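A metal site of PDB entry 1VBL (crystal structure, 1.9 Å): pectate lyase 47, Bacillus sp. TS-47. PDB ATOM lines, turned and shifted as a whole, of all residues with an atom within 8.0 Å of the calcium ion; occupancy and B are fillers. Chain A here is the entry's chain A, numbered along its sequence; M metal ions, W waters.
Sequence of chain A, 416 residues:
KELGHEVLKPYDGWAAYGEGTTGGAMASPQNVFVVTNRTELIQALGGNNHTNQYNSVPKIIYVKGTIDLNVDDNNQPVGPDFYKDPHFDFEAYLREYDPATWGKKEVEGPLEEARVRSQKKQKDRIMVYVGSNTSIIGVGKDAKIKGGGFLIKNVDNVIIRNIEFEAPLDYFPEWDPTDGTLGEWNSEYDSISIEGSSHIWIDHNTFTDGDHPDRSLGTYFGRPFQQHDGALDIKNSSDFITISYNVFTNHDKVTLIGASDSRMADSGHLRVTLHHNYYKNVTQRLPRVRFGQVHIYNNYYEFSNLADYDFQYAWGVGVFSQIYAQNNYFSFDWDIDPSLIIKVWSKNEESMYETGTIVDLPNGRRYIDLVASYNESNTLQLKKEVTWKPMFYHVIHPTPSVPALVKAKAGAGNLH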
ATOM      1  N   SER A 187      32.431 -21.660   6.424  1.00  0.00           N
ATOM      2  CA  SER A 187      32.286 -22.786   7.324  1.00  0.00           C
ATOM      3  C   SER A 187      30.822 -23.084   7.631  1.00  0.00           C
ATOM      4  O   SER A 187      29.942 -22.278   7.372  1.00  0.00           O
ATOM      5  CB  SER A 187      33.071 -22.541   8.598  1.00  0.00           C
ATOM      6  OG  SER A 187      34.461 -22.586   8.311  1.00  0.00           O
ATOM      7  N   GLU A 188      30.594 -24.254   8.218  1.00  0.00           N
ATOM      8  CA  GLU A 188      29.247 -24.735   8.515  1.00  0.00           C
ATOM      9  C   GLU A 188      28.751 -24.687   9.951  1.00  0.00           C
ATOM     10  O   GLU A 188      27.549 -24.629  10.190  1.00  0.00           O
ATOM     11  CB  GLU A 188      29.147 -26.178   8.009  1.00  0.00           C
ATOM     12  CG  GLU A 188      27.942 -26.960   8.494  1.00  0.00           C
ATOM     13  CD  GLU A 188      26.807 -26.988   7.497  1.00  0.00           C
ATOM     14  OE1 GLU A 188      25.750 -27.560   7.828  1.00  0.00           O
ATOM     15  OE2 GLU A 188      26.977 -26.453   6.387  1.00  0.00           O
ATOM     16  N   TYR A 189      29.659 -24.698  10.913  1.00  0.00           N
ATOM     17  CA  TYR A 189      29.251 -24.779  12.315  1.00  0.00           C
ATOM     18  C   TYR A 189      28.995 -23.511  13.105  1.00  0.00           C
ATOM     19  O   TYR A 189      29.802 -22.580  13.102  1.00  0.00           O
ATOM     20  CB  TYR A 189      30.260 -25.667  13.061  1.00  0.00           C
ATOM     21  CG  TYR A 189      30.650 -26.893  12.264  1.00  0.00           C
ATOM     22  CD1 TYR A 189      29.677 -27.775  11.776  1.00  0.00           C
ATOM     23  CD2 TYR A 189      31.985 -27.140  11.940  1.00  0.00           C
ATOM     24  CE1 TYR A 189      30.020 -28.866  10.977  1.00  0.00           C
ATOM     25  CE2 TYR A 189      32.347 -28.237  11.131  1.00  0.00           C
ATOM     26  CZ  TYR A 189      31.353 -29.091  10.658  1.00  0.00           C
ATOM     27  OH  TYR A 189      31.686 -30.152   9.842  1.00  0.00           O
ATOM     28  N   ASP A 190      27.866 -23.506  13.809  1.00  0.00           N
ATOM     29  CA  ASP A 190      27.457 -22.398  14.682  1.00  0.00           C
ATOM     30  C   ASP A 190      27.406 -22.950  16.099  1.00  0.00           C
ATOM     31  O   ASP A 190      27.251 -24.162  16.281  1.00  0.00           O
ATOM     32  CB  ASP A 190      26.044 -21.913  14.338  1.00  0.00           C
ATOM     33  CG  ASP A 190      25.806 -21.794  12.866  1.00  0.00           C
ATOM     34  OD1 ASP A 190      26.654 -21.183  12.181  1.00  0.00           O
ATOM     35  OD2 ASP A 190      24.764 -22.304  12.399  1.00  0.00           O
ATOM     36  N   SER A 191      27.520 -22.083  17.096  1.00  0.00           N
ATOM     37  CA  SER A 191      27.433 -22.551  18.472  1.00  0.00           C
ATOM     38  C   SER A 191      26.003 -23.034  18.711  1.00  0.00           C
ATOM     39  O   SER A 191      25.782 -24.031  19.411  1.00  0.00           O
ATOM     40  CB  SER A 191      27.786 -21.418  19.452  1.00  0.00           C
ATOM     41  OG  SER A 191      29.180 -21.163  19.415  1.00  0.00           O
ATOM     42  N   ILE A 192      25.053 -22.328  18.130  1.00  0.00           N
ATOM     43  CA  ILE A 192      23.641 -22.694  18.227  1.00  0.00           C
ATOM     44  C   ILE A 192      22.986 -22.420  16.878  1.00  0.00           C
ATOM     45  O   ILE A 192      23.023 -21.298  16.373  1.00  0.00           O
ATOM     46  CB  ILE A 192      22.889 -21.878  19.319  1.00  0.00           C
ATOM     47  CG1 ILE A 192      23.420 -22.254  20.702  1.00  0.00           C
ATOM     48  CG2 ILE A 192      21.381 -22.169  19.235  1.00  0.00           C
ATOM     49  CD1 ILE A 192      22.690 -21.558  21.849  1.00  0.00           C
ATOM     50  N   SER A 193      22.401 -23.465  16.302  1.00  0.00           N
ATOM     51  CA  SER A 193      21.739 -23.354  15.026  1.00  0.00           C
ATOM     52  C   SER A 193      20.280 -23.769  15.196  1.00  0.00           C
ATOM     53  O   SER A 193      19.984 -24.909  15.559  1.00  0.00           O
ATOM     54  CB  SER A 193      22.424 -24.269  13.995  1.00  0.00           C
ATOM     55  OG  SER A 193      21.731 -24.247  12.765  1.00  0.00           O
ATOM     56  N   ILE A 194      19.381 -22.833  14.946  1.00  0.00           N
ATOM     57  CA  ILE A 194      17.952 -23.074  15.081  1.00  0.00           C
ATOM     58  C   ILE A 194      17.348 -23.194  13.680  1.00  0.00           C
ATOM     59  O   ILE A 194      17.328 -22.217  12.914  1.00  0.00           O
ATOM     60  CB  ILE A 194      17.286 -21.906  15.852  1.00  0.00           C
ATOM     61  CG1 ILE A 194      17.949 -21.772  17.227  1.00  0.00           C
ATOM     62  CG2 ILE A 194      15.793 -22.135  15.975  1.00  0.00           C
ATOM     63  CD1 ILE A 194      17.497 -20.562  18.036  1.00  0.00           C
ATOM     64  N   GLU A 195      16.864 -24.387  13.352  1.00  0.00           N
ATOM     65  CA  GLU A 195      16.291 -24.635  12.027  1.00  0.00           C
ATOM     66  C   GLU A 195      14.934 -25.313  12.127  1.00  0.00           C
ATOM     67  O   GLU A 195      14.794 -26.360  12.763  1.00  0.00           O
ATOM     68  CB  GLU A 195      17.252 -25.534  11.215  1.00  0.00           C
ATOM     69  CG  GLU A 195      18.714 -25.114  11.326  1.00  0.00           C
ATOM     70  CD  GLU A 195      19.675 -26.101  10.669  1.00  0.00           C
ATOM     71  OE1 GLU A 195      20.888 -25.996  10.920  1.00  0.00           O
ATOM     72  OE2 GLU A 195      19.214 -26.978   9.898  1.00  0.00           O
ATOM     73  N   HIS A 228      35.047 -20.254  11.259  1.00  0.00           N
ATOM     74  CA  HIS A 228      33.870 -20.049  12.103  1.00  0.00           C
ATOM     75  C   HIS A 228      32.697 -19.696  11.222  1.00  0.00           C
ATOM     76  O   HIS A 228      32.872 -19.294  10.071  1.00  0.00           O
ATOM     77  CB  HIS A 228      34.063 -18.872  13.069  1.00  0.00           C
ATOM     78  CG  HIS A 228      35.152 -19.071  14.081  1.00  0.00           C
ATOM     79  ND1 HIS A 228      36.320 -18.338  14.057  1.00  0.00           N
ATOM     80  CD2 HIS A 228      35.232 -19.885  15.156  1.00  0.00           C
ATOM     81  CE1 HIS A 228      37.070 -18.697  15.082  1.00  0.00           C
ATOM     82  NE2 HIS A 228      36.436 -19.627  15.758  1.00  0.00           N
ATOM     83  N   ASP A 229      31.494 -19.838  11.755  1.00  0.00           N
ATOM     84  CA  ASP A 229      30.320 -19.420  11.017  1.00  0.00           C
ATOM     85  C   ASP A 229      29.497 -18.588  11.989  1.00  0.00           C
ATOM     86  O   ASP A 229      30.015 -17.633  12.559  1.00  0.00           O
ATOM     87  CB  ASP A 229      29.528 -20.602  10.465  1.00  0.00           C
ATOM     88  CG  ASP A 229      28.577 -20.172   9.348  1.00  0.00           C
ATOM     89  OD1 ASP A 229      28.984 -19.332   8.513  1.00  0.00           O
ATOM     90  OD2 ASP A 229      27.445 -20.678   9.286  1.00  0.00           O
ATOM     91  N   GLY A 230      28.236 -18.936  12.203  1.00  0.00           N
ATOM     92  CA  GLY A 230      27.430 -18.141  13.097  1.00  0.00           C
ATOM     93  C   GLY A 230      27.557 -18.453  14.576  1.00  0.00           C
ATOM     94  O   GLY A 230      27.993 -19.532  14.974  1.00  0.00           O
ATOM     95  N   ALA A 231      27.199 -17.476  15.414  1.00  0.00           N
ATOM     96  CA  ALA A 231      27.227 -17.689  16.854  1.00  0.00           C
ATOM     97  C   ALA A 231      25.862 -18.301  17.156  1.00  0.00           C
ATOM     98  O   ALA A 231      25.749 -19.340  17.808  1.00  0.00           O
ATOM     99  CB  ALA A 231      27.382 -16.356  17.588  1.00  0.00           C
ATOM    100  N   LEU A 232      24.829 -17.648  16.646  1.00  0.00           N
ATOM    101  CA  LEU A 232      23.452 -18.075  16.854  1.00  0.00           C
ATOM    102  C   LEU A 232      22.660 -17.756  15.595  1.00  0.00           C
ATOM    103  O   LEU A 232      22.251 -16.610  15.386  1.00  0.00           O
ATOM    104  CB  LEU A 232      22.868 -17.321  18.049  1.00  0.00           C
ATOM    105  CG  LEU A 232      21.590 -17.826  18.734  1.00  0.00           C
ATOM    106  CD1 LEU A 232      21.225 -16.854  19.849  1.00  0.00           C
ATOM    107  CD2 LEU A 232      20.461 -17.949  17.734  1.00  0.00           C
ATOM    108  N   ASP A 233      22.439 -18.759  14.757  1.00  0.00           N
ATOM    109  CA  ASP A 233      21.690 -18.549  13.526  1.00  0.00           C
ATOM    110  C   ASP A 233      20.293 -19.130  13.591  1.00  0.00           C
ATOM    111  O   ASP A 233      20.066 -20.154  14.246  1.00  0.00           O
ATOM    112  CB  ASP A 233      22.450 -19.115  12.321  1.00  0.00           C
ATOM    113  CG  ASP A 233      23.679 -18.283  11.978  1.00  0.00           C
ATOM    114  OD1 ASP A 233      23.719 -17.092  12.331  1.00  0.00           O
ATOM    115  OD2 ASP A 233      24.613 -18.824  11.347  1.00  0.00           O
ATOM    116  N   ILE A 234      19.363 -18.466  12.911  1.00  0.00           N
ATOM    117  CA  ILE A 234      17.959 -18.853  12.894  1.00  0.00           C
ATOM    118  C   ILE A 234      17.485 -18.895  11.447  1.00  0.00           C
ATOM    119  O   ILE A 234      17.565 -17.900  10.735  1.00  0.00           O
ATOM    120  CB  ILE A 234      17.138 -17.822  13.688  1.00  0.00           C
ATOM    121  CG1 ILE A 234      17.671 -17.742  15.128  1.00  0.00           C
ATOM    122  CG2 ILE A 234      15.652 -18.180  13.667  1.00  0.00           C
ATOM    123  CD1 ILE A 234      17.090 -16.616  15.948  1.00  0.00           C
ATOM    124  N   LYS A 235      16.976 -20.046  11.024  1.00  0.00           N
ATOM    125  CA  LYS A 235      16.528 -20.167   9.633  1.00  0.00           C
ATOM    126  C   LYS A 235      15.470 -21.237   9.400  1.00  0.00           C
ATOM    127  O   LYS A 235      15.012 -21.915  10.324  1.00  0.00           O
ATOM    128  CB  LYS A 235      17.728 -20.459   8.731  1.00  0.00           C
ATOM    129  CG  LYS A 235      18.393 -21.804   9.023  1.00  0.00           C
ATOM    130  CD  LYS A 235      19.586 -22.056   8.102  1.00  0.00           C
ATOM    131  CE  LYS A 235      20.207 -23.416   8.368  1.00  0.00           C
ATOM    132  NZ  LYS A 235      21.387 -23.688   7.495  1.00  0.00           N
ATOM    133  N   LYS A 253      30.492 -13.198  12.030  1.00  0.00           N
ATOM    134  CA  LYS A 253      29.064 -13.267  11.701  1.00  0.00           C
ATOM    135  C   LYS A 253      28.268 -13.795  12.894  1.00  0.00           C
ATOM    136  O   LYS A 253      28.225 -15.002  13.129  1.00  0.00           O
ATOM    137  CB  LYS A 253      28.859 -14.171  10.486  1.00  0.00           C
ATOM    138  CG  LYS A 253      29.640 -13.741   9.251  1.00  0.00           C
ATOM    139  CD  LYS A 253      29.363 -14.663   8.079  1.00  0.00           C
ATOM    140  CE  LYS A 253      30.040 -14.185   6.804  1.00  0.00           C
ATOM    141  NZ  LYS A 253      31.526 -14.343   6.841  1.00  0.00           N
ATOM    142  N   VAL A 254      27.625 -12.899  13.617  1.00  0.00           N
ATOM    143  CA  VAL A 254      26.890 -13.273  14.816  1.00  0.00           C
ATOM    144  C   VAL A 254      25.550 -13.977  14.656  1.00  0.00           C
ATOM    145  O   VAL A 254      25.433 -15.173  14.924  1.00  0.00           O
ATOM    146  CB  VAL A 254      26.693 -12.048  15.740  1.00  0.00           C
ATOM    147  CG1 VAL A 254      25.961 -12.452  17.014  1.00  0.00           C
ATOM    148  CG2 VAL A 254      28.049 -11.441  16.083  1.00  0.00           C
ATOM    149  N   LEU A 256      22.221 -14.665  12.069  1.00  0.00           N
ATOM    150  CA  LEU A 256      21.493 -14.628  10.821  1.00  0.00           C
ATOM    151  C   LEU A 256      20.053 -15.045  11.132  1.00  0.00           C
ATOM    152  O   LEU A 256      19.817 -16.000  11.873  1.00  0.00           O
ATOM    153  CB  LEU A 256      22.114 -15.615   9.831  1.00  0.00           C
ATOM    154  CG  LEU A 256      21.536 -15.712   8.416  1.00  0.00           C
ATOM    155  CD1 LEU A 256      21.755 -14.400   7.675  1.00  0.00           C
ATOM    156  CD2 LEU A 256      22.220 -16.857   7.689  1.00  0.00           C
ATOM    157  N   ALA A 259      17.895 -17.349   6.003  1.00  0.00           N
ATOM    158  CA  ALA A 259      19.090 -17.593   5.196  1.00  0.00           C
ATOM    159  C   ALA A 259      18.952 -17.399   3.684  1.00  0.00           C
ATOM    160  O   ALA A 259      19.942 -17.542   2.964  1.00  0.00           O
ATOM    161  CB  ALA A 259      19.623 -18.993   5.475  1.00  0.00           C
ATOM    162  N   ARG A 285      25.971  -8.786  11.241  1.00  0.00           N
ATOM    163  CA  ARG A 285      24.764  -9.559  11.531  1.00  0.00           C
ATOM    164  C   ARG A 285      24.369  -9.476  13.003  1.00  0.00           C
ATOM    165  O   ARG A 285      24.423 -10.468  13.722  1.00  0.00           O
ATOM    166  CB  ARG A 285      24.966 -11.037  11.152  1.00  0.00           C
ATOM    167  CG  ARG A 285      25.350 -11.262   9.692  1.00  0.00           C
ATOM    168  CD  ARG A 285      25.466 -12.748   9.394  1.00  0.00           C
ATOM    169  NE  ARG A 285      25.744 -13.013   7.986  1.00  0.00           N
ATOM    170  CZ  ARG A 285      25.851 -14.234   7.467  1.00  0.00           C
ATOM    171  NH1 ARG A 285      25.711 -15.299   8.236  1.00  0.00           N
ATOM    172  NH2 ARG A 285      26.107 -14.382   6.171  1.00  0.00           N
HETATM  173 CA    CA M   1      25.027 -21.000  10.112  1.00  0.00          CA
HETATM  174  O   HOH W   1      22.498 -21.627   9.825  1.00  0.00           O
HETATM  175  O   HOH W   2      24.903 -20.152   7.747  1.00  0.00           O
HETATM  176  O   HOH W   3      26.105 -23.016   9.416  1.00  0.00           O
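Water W3 binds the calcium ion (2.4 Å). Water W2 binds the calcium ion, 2.5 Å away. OD2 of Asp 233 is bound to the calcium ion, at 2.5 Å. The side-chain carboxylate (OD2) of Asp 229 binds the calcium ion. The calcium ion is bound by water W1 (2.6 Å). OD1 of Asp 190 is bound to the calcium ion. The calcium ion is bound by OD2 of Asp 190, 2.6 Å away.
Within 4 Å of the calcium ion: Asp 190, Asp 229 and Asp 233. Along chain A the residues within 4 Å of the calcium ion span positions 190 to 233.
The side-chain carboxylate of Asp 233 is in hydrogen-bond range of the backbone NH of Leu 256, 2.9 Å away. The backbone NH of Asp 229 lies close to the backbone carbonyl oxygen of Tyr 189. The backbone carbonyl oxygen (O) of Asp 233 sits at hydrogen-bond distance from the backbone NH (N) of Ile 194. N of Asp 233 lies within hydrogen-bond range of O of Ile 192 (3.1 Å). The side-chain carboxylate (OD1) of Asp 190 lies close to the backbone NH (N) of Gly 230 (2.7 Å).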
